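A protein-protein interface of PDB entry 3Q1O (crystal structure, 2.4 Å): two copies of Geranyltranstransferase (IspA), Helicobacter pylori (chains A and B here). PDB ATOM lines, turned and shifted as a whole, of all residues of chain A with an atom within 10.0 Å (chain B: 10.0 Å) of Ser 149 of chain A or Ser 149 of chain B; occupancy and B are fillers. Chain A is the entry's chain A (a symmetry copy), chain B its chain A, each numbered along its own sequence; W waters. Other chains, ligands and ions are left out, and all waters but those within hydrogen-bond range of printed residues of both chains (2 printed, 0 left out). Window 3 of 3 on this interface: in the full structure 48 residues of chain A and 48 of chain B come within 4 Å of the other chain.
Of the printed residues of chain B, Ser 143 of chain A touches Val 153 (3.4 Å), Ile 156 (3.8 Å) and Lys 157 (3.3 Å). Of the printed residues of chain B, His 150 of chain A touches Ser 149 (3.4 Å). Ile 152 of chain A touches just one residue of chain B: Val 153. Leu 155 of chain A touches none of the printed residues of chain B. Gln 79 of chain B touches none of the printed residues of chain A. Of chain A, only Ser 149, His 150 and Val 153 come within 4 Å of Ser 149 of chain B. The nearest printed residue of chain B that does not touch His 150 of chain A is Val 153 of chain B (5.8 Å).
Among the printed residues, merely in contact across the chains: Ser 143 of chain A with Val 153 of chain B (3.4 Å), Ser 143 of chain A with Ile 156 of chain B (3.8 Å), Ser 143 of chain A with Lys 157 of chain B (3.3 Å), Asn 144 of chain A with Lys 157 of chain B (3.5 Å), Ser 149 of chain A with Ser 149 of chain B (3.5 Å), Ser 149 of chain A with His 150 of chain B (3.4 Å), Ser 149 of chain A with Val 153 of chain B (3.9 Å), His 150 of chain A with Ser 149 of chain B (3.4 Å), Ile 152 of chain A with Val 153 of chain B (3.8 Å), Val 153 of chain A with Ser 143 of chain B (3.4 Å), Val 153 of chain A with Ser 149 of chain B (3.9 Å), Val 153 of chain A with Ile 152 of chain B (3.8 Å), Ile 156 of chain A with Ser 143 of chain B (3.8 Å), Ile 156 of chain A with Ile 156 of chain B (3.7 Å), Lys 157 of chain A with Ser 143 of chain B (3.3 Å) and Lys 157 of chain A with Asn 144 of chain B (3.5 Å).
Water W2 bridges the side-chain amino group of Lys 157 of chain B (3.1 Å) and the backbone carbonyl oxygen of Asn 144 of chain A (3.3 Å). Water W1 bridges NZ of Lys 157 of chain A and O of Asn 144 of chain B.
Ser 143 of chain A touches Ile 156 of chain B, and with the chains exchanged Ile 156 of chain A touches Ser 143 of chain B. Ser 143 of chain A touches Lys 157 of chain B, and with the chains exchanged Lys 157 of chain A touches Ser 143 of chain B. Ser 149 of chain A touches its own counterpart, Ser 149 of chain B. Ile 156 of chain A touches its own counterpart, Ile 156 of chain B.
Along chain A the printed residues that touch a printed residue of chain B span positions 143 to 157. Among the printed residues, no Asp or Glu carboxylate lies within 4 Å of a Lys or Arg side-chain nitrogen of the other chain.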
ATOM      1  N   GLN A  79      23.815 -12.961 -34.655  1.00  0.00           N
ATOM      2  CA  GLN A  79      22.907 -14.098 -34.553  1.00  0.00           C
ATOM      3  C   GLN A  79      21.696 -14.000 -35.488  1.00  0.00           C
ATOM      4  O   GLN A  79      20.782 -14.822 -35.391  1.00  0.00           O
ATOM      5  CB  GLN A  79      22.419 -14.228 -33.109  1.00  0.00           C
ATOM      6  CG  GLN A  79      23.452 -13.892 -32.046  1.00  0.00           C
ATOM      7  CD  GLN A  79      24.098 -15.121 -31.457  1.00  0.00           C
ATOM      8  OE1 GLN A  79      24.087 -15.309 -30.241  1.00  0.00           O
ATOM      9  NE2 GLN A  79      24.660 -15.976 -32.314  1.00  0.00           N
ATOM     10  N   LEU A 142      14.528 -25.382 -35.891  1.00  0.00           N
ATOM     11  CA  LEU A 142      14.734 -24.912 -34.536  1.00  0.00           C
ATOM     12  C   LEU A 142      15.997 -25.514 -33.922  1.00  0.00           C
ATOM     13  O   LEU A 142      16.823 -24.788 -33.370  1.00  0.00           O
ATOM     14  CB  LEU A 142      13.503 -25.242 -33.698  1.00  0.00           C
ATOM     15  CG  LEU A 142      12.918 -24.199 -32.759  1.00  0.00           C
ATOM     16  CD1 LEU A 142      13.107 -22.822 -33.276  1.00  0.00           C
ATOM     17  CD2 LEU A 142      11.446 -24.483 -32.601  1.00  0.00           C
ATOM     18  N   SER A 143      16.168 -26.827 -34.069  1.00  0.00           N
ATOM     19  CA  SER A 143      17.338 -27.523 -33.529  1.00  0.00           C
ATOM     20  C   SER A 143      18.646 -27.182 -34.243  1.00  0.00           C
ATOM     21  O   SER A 143      19.723 -27.376 -33.674  1.00  0.00           O
ATOM     22  CB  SER A 143      17.122 -29.038 -33.510  1.00  0.00           C
ATOM     23  OG  SER A 143      16.938 -29.550 -34.814  1.00  0.00           O
ATOM     24  N   ASN A 144      18.548 -26.668 -35.468  1.00  0.00           N
ATOM     25  CA  ASN A 144      19.722 -26.230 -36.218  1.00  0.00           C
ATOM     26  C   ASN A 144      20.108 -24.757 -36.068  1.00  0.00           C
ATOM     27  O   ASN A 144      21.117 -24.313 -36.623  1.00  0.00           O
ATOM     28  CB  ASN A 144      19.595 -26.627 -37.692  1.00  0.00           C
ATOM     29  CG  ASN A 144      19.853 -28.108 -37.909  1.00  0.00           C
ATOM     30  OD1 ASN A 144      20.953 -28.608 -37.659  1.00  0.00           O
ATOM     31  ND2 ASN A 144      18.835 -28.822 -38.355  1.00  0.00           N
ATOM     32  N   ALA A 145      19.310 -24.000 -35.322  1.00  0.00           N
ATOM     33  CA  ALA A 145      19.623 -22.604 -35.040  1.00  0.00           C
ATOM     34  C   ALA A 145      20.732 -22.530 -33.993  1.00  0.00           C
ATOM     35  O   ALA A 145      20.645 -23.160 -32.938  1.00  0.00           O
ATOM     36  CB  ALA A 145      18.387 -21.864 -34.575  1.00  0.00           C
ATOM     37  N   LEU A 146      21.776 -21.763 -34.293  1.00  0.00           N
ATOM     38  CA  LEU A 146      22.974 -21.744 -33.462  1.00  0.00           C
ATOM     39  C   LEU A 146      22.857 -20.719 -32.341  1.00  0.00           C
ATOM     40  O   LEU A 146      23.505 -19.668 -32.358  1.00  0.00           O
ATOM     41  CB  LEU A 146      24.231 -21.517 -34.314  1.00  0.00           C
ATOM     42  CG  LEU A 146      24.472 -22.525 -35.453  1.00  0.00           C
ATOM     43  CD1 LEU A 146      25.430 -21.977 -36.513  1.00  0.00           C
ATOM     44  CD2 LEU A 146      24.959 -23.870 -34.918  1.00  0.00           C
ATOM     45  N   LEU A 147      21.993 -21.026 -31.382  1.00  0.00           N
ATOM     46  CA  LEU A 147      21.938 -20.285 -30.136  1.00  0.00           C
ATOM     47  C   LEU A 147      22.316 -21.263 -29.043  1.00  0.00           C
ATOM     48  O   LEU A 147      22.503 -22.452 -29.314  1.00  0.00           O
ATOM     49  CB  LEU A 147      20.534 -19.729 -29.874  1.00  0.00           C
ATOM     50  CG  LEU A 147      19.882 -18.747 -30.846  1.00  0.00           C
ATOM     51  CD1 LEU A 147      18.625 -18.212 -30.196  1.00  0.00           C
ATOM     52  CD2 LEU A 147      20.810 -17.600 -31.220  1.00  0.00           C
ATOM     53  N   GLU A 148      22.419 -20.770 -27.813  1.00  0.00           N
ATOM     54  CA  GLU A 148      22.675 -21.622 -26.663  1.00  0.00           C
ATOM     55  C   GLU A 148      21.668 -22.760 -26.577  1.00  0.00           C
ATOM     56  O   GLU A 148      20.478 -22.579 -26.853  1.00  0.00           O
ATOM     57  CB  GLU A 148      22.670 -20.805 -25.378  1.00  0.00           C
ATOM     58  CG  GLU A 148      23.928 -19.991 -25.188  1.00  0.00           C
ATOM     59  CD  GLU A 148      23.795 -18.994 -24.063  1.00  0.00           C
ATOM     60  OE1 GLU A 148      23.308 -17.871 -24.322  1.00  0.00           O
ATOM     61  OE2 GLU A 148      24.180 -19.333 -22.923  1.00  0.00           O
ATOM     62  N   SER A 149      22.172 -23.930 -26.209  1.00  0.00           N
ATOM     63  CA  SER A 149      21.399 -25.153 -26.184  1.00  0.00           C
ATOM     64  C   SER A 149      20.135 -25.067 -25.346  1.00  0.00           C
ATOM     65  O   SER A 149      19.085 -25.543 -25.777  1.00  0.00           O
ATOM     66  CB  SER A 149      22.276 -26.304 -25.711  1.00  0.00           C
ATOM     67  OG  SER A 149      22.994 -26.850 -26.793  1.00  0.00           O
ATOM     68  N   HIS A 150      20.225 -24.438 -24.174  1.00  0.00           N
ATOM     69  CA  HIS A 150      19.081 -24.363 -23.262  1.00  0.00           C
ATOM     70  C   HIS A 150      17.982 -23.456 -23.799  1.00  0.00           C
ATOM     71  O   HIS A 150      16.809 -23.638 -23.471  1.00  0.00           O
ATOM     72  CB  HIS A 150      19.506 -23.944 -21.846  1.00  0.00           C
ATOM     73  CG  HIS A 150      20.057 -22.556 -21.763  1.00  0.00           C
ATOM     74  ND1 HIS A 150      21.363 -22.253 -22.087  1.00  0.00           N
ATOM     75  CD2 HIS A 150      19.481 -21.389 -21.388  1.00  0.00           C
ATOM     76  CE1 HIS A 150      21.568 -20.957 -21.917  1.00  0.00           C
ATOM     77  NE2 HIS A 150      20.441 -20.410 -21.496  1.00  0.00           N
ATOM     78  N   ILE A 151      18.373 -22.490 -24.628  1.00  0.00           N
ATOM     79  CA  ILE A 151      17.422 -21.621 -25.319  1.00  0.00           C
ATOM     80  C   ILE A 151      16.663 -22.428 -26.377  1.00  0.00           C
ATOM     81  O   ILE A 151      15.432 -22.403 -26.408  1.00  0.00           O
ATOM     82  CB  ILE A 151      18.117 -20.363 -25.926  1.00  0.00           C
ATOM     83  CG1 ILE A 151      18.620 -19.447 -24.800  1.00  0.00           C
ATOM     84  CG2 ILE A 151      17.176 -19.605 -26.883  1.00  0.00           C
ATOM     85  CD1 ILE A 151      19.598 -18.361 -25.254  1.00  0.00           C
ATOM     86  N   ILE A 152      17.402 -23.161 -27.209  1.00  0.00           N
ATOM     87  CA  ILE A 152      16.821 -24.025 -28.235  1.00  0.00           C
ATOM     88  C   ILE A 152      15.804 -25.013 -27.646  1.00  0.00           C
ATOM     89  O   ILE A 152      14.686 -25.118 -28.154  1.00  0.00           O
ATOM     90  CB  ILE A 152      17.915 -24.750 -29.072  1.00  0.00           C
ATOM     91  CG1 ILE A 152      18.827 -23.737 -29.772  1.00  0.00           C
ATOM     92  CG2 ILE A 152      17.300 -25.697 -30.106  1.00  0.00           C
ATOM     93  CD1 ILE A 152      18.125 -22.693 -30.629  1.00  0.00           C
ATOM     94  N   VAL A 153      16.174 -25.682 -26.552  1.00  0.00           N
ATOM     95  CA  VAL A 153      15.285 -26.633 -25.876  1.00  0.00           C
ATOM     96  C   VAL A 153      13.985 -25.949 -25.445  1.00  0.00           C
ATOM     97  O   VAL A 153      12.892 -26.479 -25.670  1.00  0.00           O
ATOM     98  CB  VAL A 153      15.974 -27.310 -24.652  1.00  0.00           C
ATOM     99  CG1 VAL A 153      14.968 -28.020 -23.751  1.00  0.00           C
ATOM    100  CG2 VAL A 153      17.037 -28.287 -25.111  1.00  0.00           C
ATOM    101  N   GLU A 154      14.123 -24.760 -24.858  1.00  0.00           N
ATOM    102  CA  GLU A 154      12.992 -23.978 -24.385  1.00  0.00           C
ATOM    103  C   GLU A 154      12.088 -23.525 -25.541  1.00  0.00           C
ATOM    104  O   GLU A 154      10.862 -23.522 -25.409  1.00  0.00           O
ATOM    105  CB  GLU A 154      13.486 -22.794 -23.538  1.00  0.00           C
ATOM    106  CG  GLU A 154      12.415 -22.073 -22.713  1.00  0.00           C
ATOM    107  CD  GLU A 154      11.653 -22.990 -21.756  1.00  0.00           C
ATOM    108  OE1 GLU A 154      12.287 -23.831 -21.075  1.00  0.00           O
ATOM    109  OE2 GLU A 154      10.409 -22.855 -21.678  1.00  0.00           O
ATOM    110  N   LEU A 155      12.693 -23.184 -26.677  1.00  0.00           N
ATOM    111  CA  LEU A 155      11.938 -22.777 -27.855  1.00  0.00           C
ATOM    112  C   LEU A 155      11.092 -23.923 -28.414  1.00  0.00           C
ATOM    113  O   LEU A 155       9.926 -23.734 -28.779  1.00  0.00           O
ATOM    114  CB  LEU A 155      12.884 -22.230 -28.926  1.00  0.00           C
ATOM    115  CG  LEU A 155      13.443 -20.833 -28.639  1.00  0.00           C
ATOM    116  CD1 LEU A 155      14.474 -20.430 -29.676  1.00  0.00           C
ATOM    117  CD2 LEU A 155      12.329 -19.806 -28.581  1.00  0.00           C
ATOM    118  N   ILE A 156      11.691 -25.109 -28.451  1.00  0.00           N
ATOM    119  CA  ILE A 156      11.027 -26.321 -28.916  1.00  0.00           C
ATOM    120  C   ILE A 156       9.887 -26.710 -27.981  1.00  0.00           C
ATOM    121  O   ILE A 156       8.808 -27.069 -28.450  1.00  0.00           O
ATOM    122  CB  ILE A 156      12.060 -27.460 -29.135  1.00  0.00           C
ATOM    123  CG1 ILE A 156      13.001 -27.053 -30.272  1.00  0.00           C
ATOM    124  CG2 ILE A 156      11.376 -28.799 -29.462  1.00  0.00           C
ATOM    125  CD1 ILE A 156      14.247 -27.860 -30.377  1.00  0.00           C
ATOM    126  N   LYS A 157      10.116 -26.593 -26.672  1.00  0.00           N
ATOM    127  CA  LYS A 157       9.067 -26.795 -25.671  1.00  0.00           C
ATOM    128  C   LYS A 157       7.828 -25.954 -25.962  1.00  0.00           C
ATOM    129  O   LYS A 157       6.713 -26.467 -25.956  1.00  0.00           O
ATOM    130  CB  LYS A 157       9.567 -26.450 -24.272  1.00  0.00           C
ATOM    131  CG  LYS A 157      10.397 -27.514 -23.598  1.00  0.00           C
ATOM    132  CD  LYS A 157      10.462 -27.243 -22.102  1.00  0.00           C
ATOM    133  CE  LYS A 157      11.653 -27.922 -21.465  1.00  0.00           C
ATOM    134  NZ  LYS A 157      11.650 -27.784 -19.984  1.00  0.00           N
ATOM    135  N   VAL A 209      12.273 -15.593 -25.112  1.00  0.00           N
ATOM    136  CA  VAL A 209      13.160 -16.734 -24.877  1.00  0.00           C
ATOM    137  C   VAL A 209      14.406 -16.695 -25.785  1.00  0.00           C
ATOM    138  O   VAL A 209      15.523 -16.917 -25.309  1.00  0.00           O
ATOM    139  CB  VAL A 209      12.401 -18.087 -25.009  1.00  0.00           C
ATOM    140  CG1 VAL A 209      13.367 -19.263 -25.050  1.00  0.00           C
ATOM    141  CG2 VAL A 209      11.439 -18.260 -23.851  1.00  0.00           C
ATOM    142  N   GLN B  79      18.525 -41.572 -14.596  1.00  0.00           N
ATOM    143  CA  GLN B  79      17.990 -40.937 -15.796  1.00  0.00           C
ATOM    144  C   GLN B  79      16.981 -41.810 -16.552  1.00  0.00           C
ATOM    145  O   GLN B  79      16.570 -41.450 -17.656  1.00  0.00           O
ATOM    146  CB  GLN B  79      19.143 -40.576 -16.733  1.00  0.00           C
ATOM    147  CG  GLN B  79      20.414 -40.109 -16.044  1.00  0.00           C
ATOM    148  CD  GLN B  79      20.551 -38.606 -16.037  1.00  0.00           C
ATOM    149  OE1 GLN B  79      21.561 -38.070 -16.494  1.00  0.00           O
ATOM    150  NE2 GLN B  79      19.533 -37.910 -15.528  1.00  0.00           N
ATOM    151  N   LEU B 142      10.692 -35.120 -26.390  1.00  0.00           N
ATOM    152  CA  LEU B 142      12.135 -35.016 -26.491  1.00  0.00           C
ATOM    153  C   LEU B 142      12.659 -33.791 -25.744  1.00  0.00           C
ATOM    154  O   LEU B 142      13.596 -33.901 -24.954  1.00  0.00           O
ATOM    155  CB  LEU B 142      12.532 -34.976 -27.963  1.00  0.00           C
ATOM    156  CG  LEU B 142      13.698 -35.816 -28.461  1.00  0.00           C
ATOM    157  CD1 LEU B 142      13.833 -37.081 -27.697  1.00  0.00           C
ATOM    158  CD2 LEU B 142      13.463 -36.127 -29.916  1.00  0.00           C
ATOM    159  N   SER B 143      12.020 -32.641 -25.954  1.00  0.00           N
ATOM    160  CA  SER B 143      12.423 -31.395 -25.297  1.00  0.00           C
ATOM    161  C   SER B 143      12.153 -31.374 -23.792  1.00  0.00           C
ATOM    162  O   SER B 143      12.773 -30.589 -23.070  1.00  0.00           O
ATOM    163  CB  SER B 143      11.781 -30.180 -25.969  1.00  0.00           C
ATOM    164  OG  SER B 143      10.371 -30.224 -25.877  1.00  0.00           O
ATOM    165  N   ASN B 144      11.250 -32.238 -23.328  1.00  0.00           N
ATOM    166  CA  ASN B 144      10.965 -32.366 -21.901  1.00  0.00           C
ATOM    167  C   ASN B 144      11.772 -33.423 -21.144  1.00  0.00           C
ATOM    168  O   ASN B 144      11.634 -33.563 -19.926  1.00  0.00           O
ATOM    169  CB  ASN B 144       9.461 -32.538 -21.669  1.00  0.00           C
ATOM    170  CG  ASN B 144       8.706 -31.230 -21.832  1.00  0.00           C
ATOM    171  OD1 ASN B 144       8.918 -30.272 -21.083  1.00  0.00           O
ATOM    172  ND2 ASN B 144       7.835 -31.174 -22.824  1.00  0.00           N
ATOM    173  N   ALA B 145      12.610 -34.166 -21.861  1.00  0.00           N
ATOM    174  CA  ALA B 145      13.489 -35.146 -21.234  1.00  0.00           C
ATOM    175  C   ALA B 145      14.652 -34.429 -20.553  1.00  0.00           C
ATOM    176  O   ALA B 145      15.322 -33.594 -21.164  1.00  0.00           O
ATOM    177  CB  ALA B 145      13.991 -36.142 -22.259  1.00  0.00           C
ATOM    178  N   LEU B 146      14.882 -34.751 -19.284  1.00  0.00           N
ATOM    179  CA  LEU B 146      15.844 -34.017 -18.471  1.00  0.00           C
ATOM    180  C   LEU B 146      17.246 -34.593 -18.613  1.00  0.00           C
ATOM    181  O   LEU B 146      17.776 -35.234 -17.700  1.00  0.00           O
ATOM    182  CB  LEU B 146      15.395 -33.962 -17.002  1.00  0.00           C
ATOM    183  CG  LEU B 146      14.006 -33.355 -16.739  1.00  0.00           C
ATOM    184  CD1 LEU B 146      13.450 -33.762 -15.372  1.00  0.00           C
ATOM    185  CD2 LEU B 146      14.018 -31.835 -16.893  1.00  0.00           C
ATOM    186  N   LEU B 147      17.828 -34.385 -19.787  1.00  0.00           N
ATOM    187  CA  LEU B 147      19.237 -34.654 -20.003  1.00  0.00           C
ATOM    188  C   LEU B 147      19.880 -33.319 -20.318  1.00  0.00           C
ATOM    189  O   LEU B 147      19.183 -32.309 -20.435  1.00  0.00           O
ATOM    190  CB  LEU B 147      19.452 -35.624 -21.170  1.00  0.00           C
ATOM    191  CG  LEU B 147      18.870 -37.037 -21.136  1.00  0.00           C
ATOM    192  CD1 LEU B 147      19.450 -37.808 -22.301  1.00  0.00           C
ATOM    193  CD2 LEU B 147      19.169 -37.756 -19.829  1.00  0.00           C
ATOM    194  N   GLU B 148      21.201 -33.316 -20.465  1.00  0.00           N
ATOM    195  CA  GLU B 148      21.925 -32.122 -20.867  1.00  0.00           C
ATOM    196  C   GLU B 148      21.359 -31.533 -22.152  1.00  0.00           C
ATOM    197  O   GLU B 148      20.977 -32.262 -23.073  1.00  0.00           O
ATOM    198  CB  GLU B 148      23.410 -32.423 -21.028  1.00  0.00           C
ATOM    199  CG  GLU B 148      24.135 -32.546 -19.708  1.00  0.00           C
ATOM    200  CD  GLU B 148      25.527 -33.104 -19.874  1.00  0.00           C
ATOM    201  OE1 GLU B 148      25.670 -34.347 -19.878  1.00  0.00           O
ATOM    202  OE2 GLU B 148      26.476 -32.300 -19.998  1.00  0.00           O
ATOM    203  N   SER B 149      21.298 -30.209 -22.184  1.00  0.00           N
ATOM    204  CA  SER B 149      20.682 -29.470 -23.265  1.00  0.00           C
ATOM    205  C   SER B 149      21.245 -29.801 -24.637  1.00  0.00           C
ATOM    206  O   SER B 149      20.480 -29.958 -25.587  1.00  0.00           O
ATOM    207  CB  SER B 149      20.788 -27.976 -22.990  1.00  0.00           C
ATOM    208  OG  SER B 149      19.722 -27.551 -22.172  1.00  0.00           O
ATOM    209  N   HIS B 150      22.568 -29.937 -24.733  1.00  0.00           N
ATOM    210  CA  HIS B 150      23.213 -30.185 -26.024  1.00  0.00           C
ATOM    211  C   HIS B 150      22.912 -31.581 -26.554  1.00  0.00           C
ATOM    212  O   HIS B 150      22.925 -31.804 -27.765  1.00  0.00           O
ATOM    213  CB  HIS B 150      24.728 -29.928 -25.965  1.00  0.00           C
ATOM    214  CG  HIS B 150      25.468 -30.866 -25.065  1.00  0.00           C
ATOM    215  ND1 HIS B 150      25.532 -30.692 -23.697  1.00  0.00           N
ATOM    216  CD2 HIS B 150      26.180 -31.986 -25.335  1.00  0.00           C
ATOM    217  CE1 HIS B 150      26.252 -31.665 -23.165  1.00  0.00           C
ATOM    218  NE2 HIS B 150      26.654 -32.465 -24.137  1.00  0.00           N
ATOM    219  N   ILE B 151      22.635 -32.507 -25.638  1.00  0.00           N
ATOM    220  CA  ILE B 151      22.205 -33.858 -25.997  1.00  0.00           C
ATOM    221  C   ILE B 151      20.794 -33.808 -26.591  1.00  0.00           C
ATOM    222  O   ILE B 151      20.560 -34.343 -27.675  1.00  0.00           O
ATOM    223  CB  ILE B 151      22.299 -34.840 -24.789  1.00  0.00           C
ATOM    224  CG1 ILE B 151      23.772 -35.068 -24.412  1.00  0.00           C
ATOM    225  CG2 ILE B 151      21.589 -36.174 -25.090  1.00  0.00           C
ATOM    226  CD1 ILE B 151      23.983 -35.739 -23.054  1.00  0.00           C
ATOM    227  N   ILE B 152      19.878 -33.135 -25.893  1.00  0.00           N
ATOM    228  CA  ILE B 152      18.504 -32.954 -26.356  1.00  0.00           C
ATOM    229  C   ILE B 152      18.448 -32.340 -27.762  1.00  0.00           C
ATOM    230  O   ILE B 152      17.752 -32.867 -28.633  1.00  0.00           O
ATOM    231  CB  ILE B 152      17.650 -32.145 -25.336  1.00  0.00           C
ATOM    232  CG1 ILE B 152      17.599 -32.857 -23.979  1.00  0.00           C
ATOM    233  CG2 ILE B 152      16.229 -31.908 -25.853  1.00  0.00           C
ATOM    234  CD1 ILE B 152      17.136 -34.308 -24.009  1.00  0.00           C
ATOM    235  N   VAL B 153      19.217 -31.274 -27.989  1.00  0.00           N
ATOM    236  CA  VAL B 153      19.276 -30.612 -29.297  1.00  0.00           C
ATOM    237  C   VAL B 153      19.713 -31.597 -30.383  1.00  0.00           C
ATOM    238  O   VAL B 153      19.103 -31.661 -31.456  1.00  0.00           O
ATOM    239  CB  VAL B 153      20.215 -29.368 -29.280  1.00  0.00           C
ATOM    240  CG1 VAL B 153      20.553 -28.891 -30.691  1.00  0.00           C
ATOM    241  CG2 VAL B 153      19.591 -28.237 -28.489  1.00  0.00           C
ATOM    242  N   GLU B 154      20.750 -32.377 -30.076  1.00  0.00           N
ATOM    243  CA  GLU B 154      21.295 -33.363 -30.995  1.00  0.00           C
ATOM    244  C   GLU B 154      20.288 -34.482 -31.294  1.00  0.00           C
ATOM    245  O   GLU B 154      20.191 -34.946 -32.432  1.00  0.00           O
ATOM    246  CB  GLU B 154      22.625 -33.911 -30.453  1.00  0.00           C
ATOM    247  CG  GLU B 154      23.472 -34.710 -31.450  1.00  0.00           C
ATOM    248  CD  GLU B 154      23.818 -33.938 -32.724  1.00  0.00           C
ATOM    249  OE1 GLU B 154      24.194 -32.744 -32.635  1.00  0.00           O
ATOM    250  OE2 GLU B 154      23.724 -34.539 -33.820  1.00  0.00           O
ATOM    251  N   LEU B 155      19.517 -34.881 -30.285  1.00  0.00           N
ATOM    252  CA  LEU B 155      18.496 -35.907 -30.457  1.00  0.00           C
ATOM    253  C   LEU B 155      17.378 -35.446 -31.394  1.00  0.00           C
ATOM    254  O   LEU B 155      16.924 -36.200 -32.262  1.00  0.00           O
ATOM    255  CB  LEU B 155      17.929 -36.322 -29.099  1.00  0.00           C
ATOM    256  CG  LEU B 155      18.857 -37.201 -28.253  1.00  0.00           C
ATOM    257  CD1 LEU B 155      18.275 -37.447 -26.874  1.00  0.00           C
ATOM    258  CD2 LEU B 155      19.134 -38.519 -28.950  1.00  0.00           C
ATOM    259  N   ILE B 156      16.964 -34.195 -31.216  1.00  0.00           N
ATOM    260  CA  ILE B 156      15.934 -33.574 -32.039  1.00  0.00           C
ATOM    261  C   ILE B 156      16.410 -33.416 -33.479  1.00  0.00           C
ATOM    262  O   ILE B 156      15.653 -33.698 -34.408  1.00  0.00           O
ATOM    263  CB  ILE B 156      15.453 -32.242 -31.401  1.00  0.00           C
ATOM    264  CG1 ILE B 156      14.767 -32.561 -30.069  1.00  0.00           C
ATOM    265  CG2 ILE B 156      14.491 -31.478 -32.327  1.00  0.00           C
ATOM    266  CD1 ILE B 156      14.562 -31.391 -29.173  1.00  0.00           C
ATOM    267  N   LYS B 157      17.671 -33.015 -33.656  1.00  0.00           N
ATOM    268  CA  LYS B 157      18.299 -32.959 -34.977  1.00  0.00           C
ATOM    269  C   LYS B 157      18.166 -34.279 -35.731  1.00  0.00           C
ATOM    270  O   LYS B 157      17.764 -34.294 -36.891  1.00  0.00           O
ATOM    271  CB  LYS B 157      19.780 -32.613 -34.867  1.00  0.00           C
ATOM    272  CG  LYS B 157      20.093 -31.151 -34.672  1.00  0.00           C
ATOM    273  CD  LYS B 157      21.555 -30.889 -35.007  1.00  0.00           C
ATOM    274  CE  LYS B 157      22.056 -29.620 -34.354  1.00  0.00           C
ATOM    275  NZ  LYS B 157      23.438 -29.277 -34.788  1.00  0.00           N
ATOM    276  N   VAL B 209      23.956 -41.070 -28.790  1.00  0.00           N
ATOM    277  CA  VAL B 209      23.854 -39.655 -28.427  1.00  0.00           C
ATOM    278  C   VAL B 209      23.277 -39.461 -27.010  1.00  0.00           C
ATOM    279  O   VAL B 209      23.809 -38.664 -26.232  1.00  0.00           O
ATOM    280  CB  VAL B 209      23.049 -38.848 -29.487  1.00  0.00           C
ATOM    281  CG1 VAL B 209      22.700 -37.457 -28.976  1.00  0.00           C
ATOM    282  CG2 VAL B 209      23.845 -38.733 -30.771  1.00  0.00           C
HETATM  283  O   HOH W   1      11.144 -30.564 -18.614  1.00  0.00           O
HETATM  284  O   HOH W   2      23.435 -26.675 -36.544  1.00  0.00           O
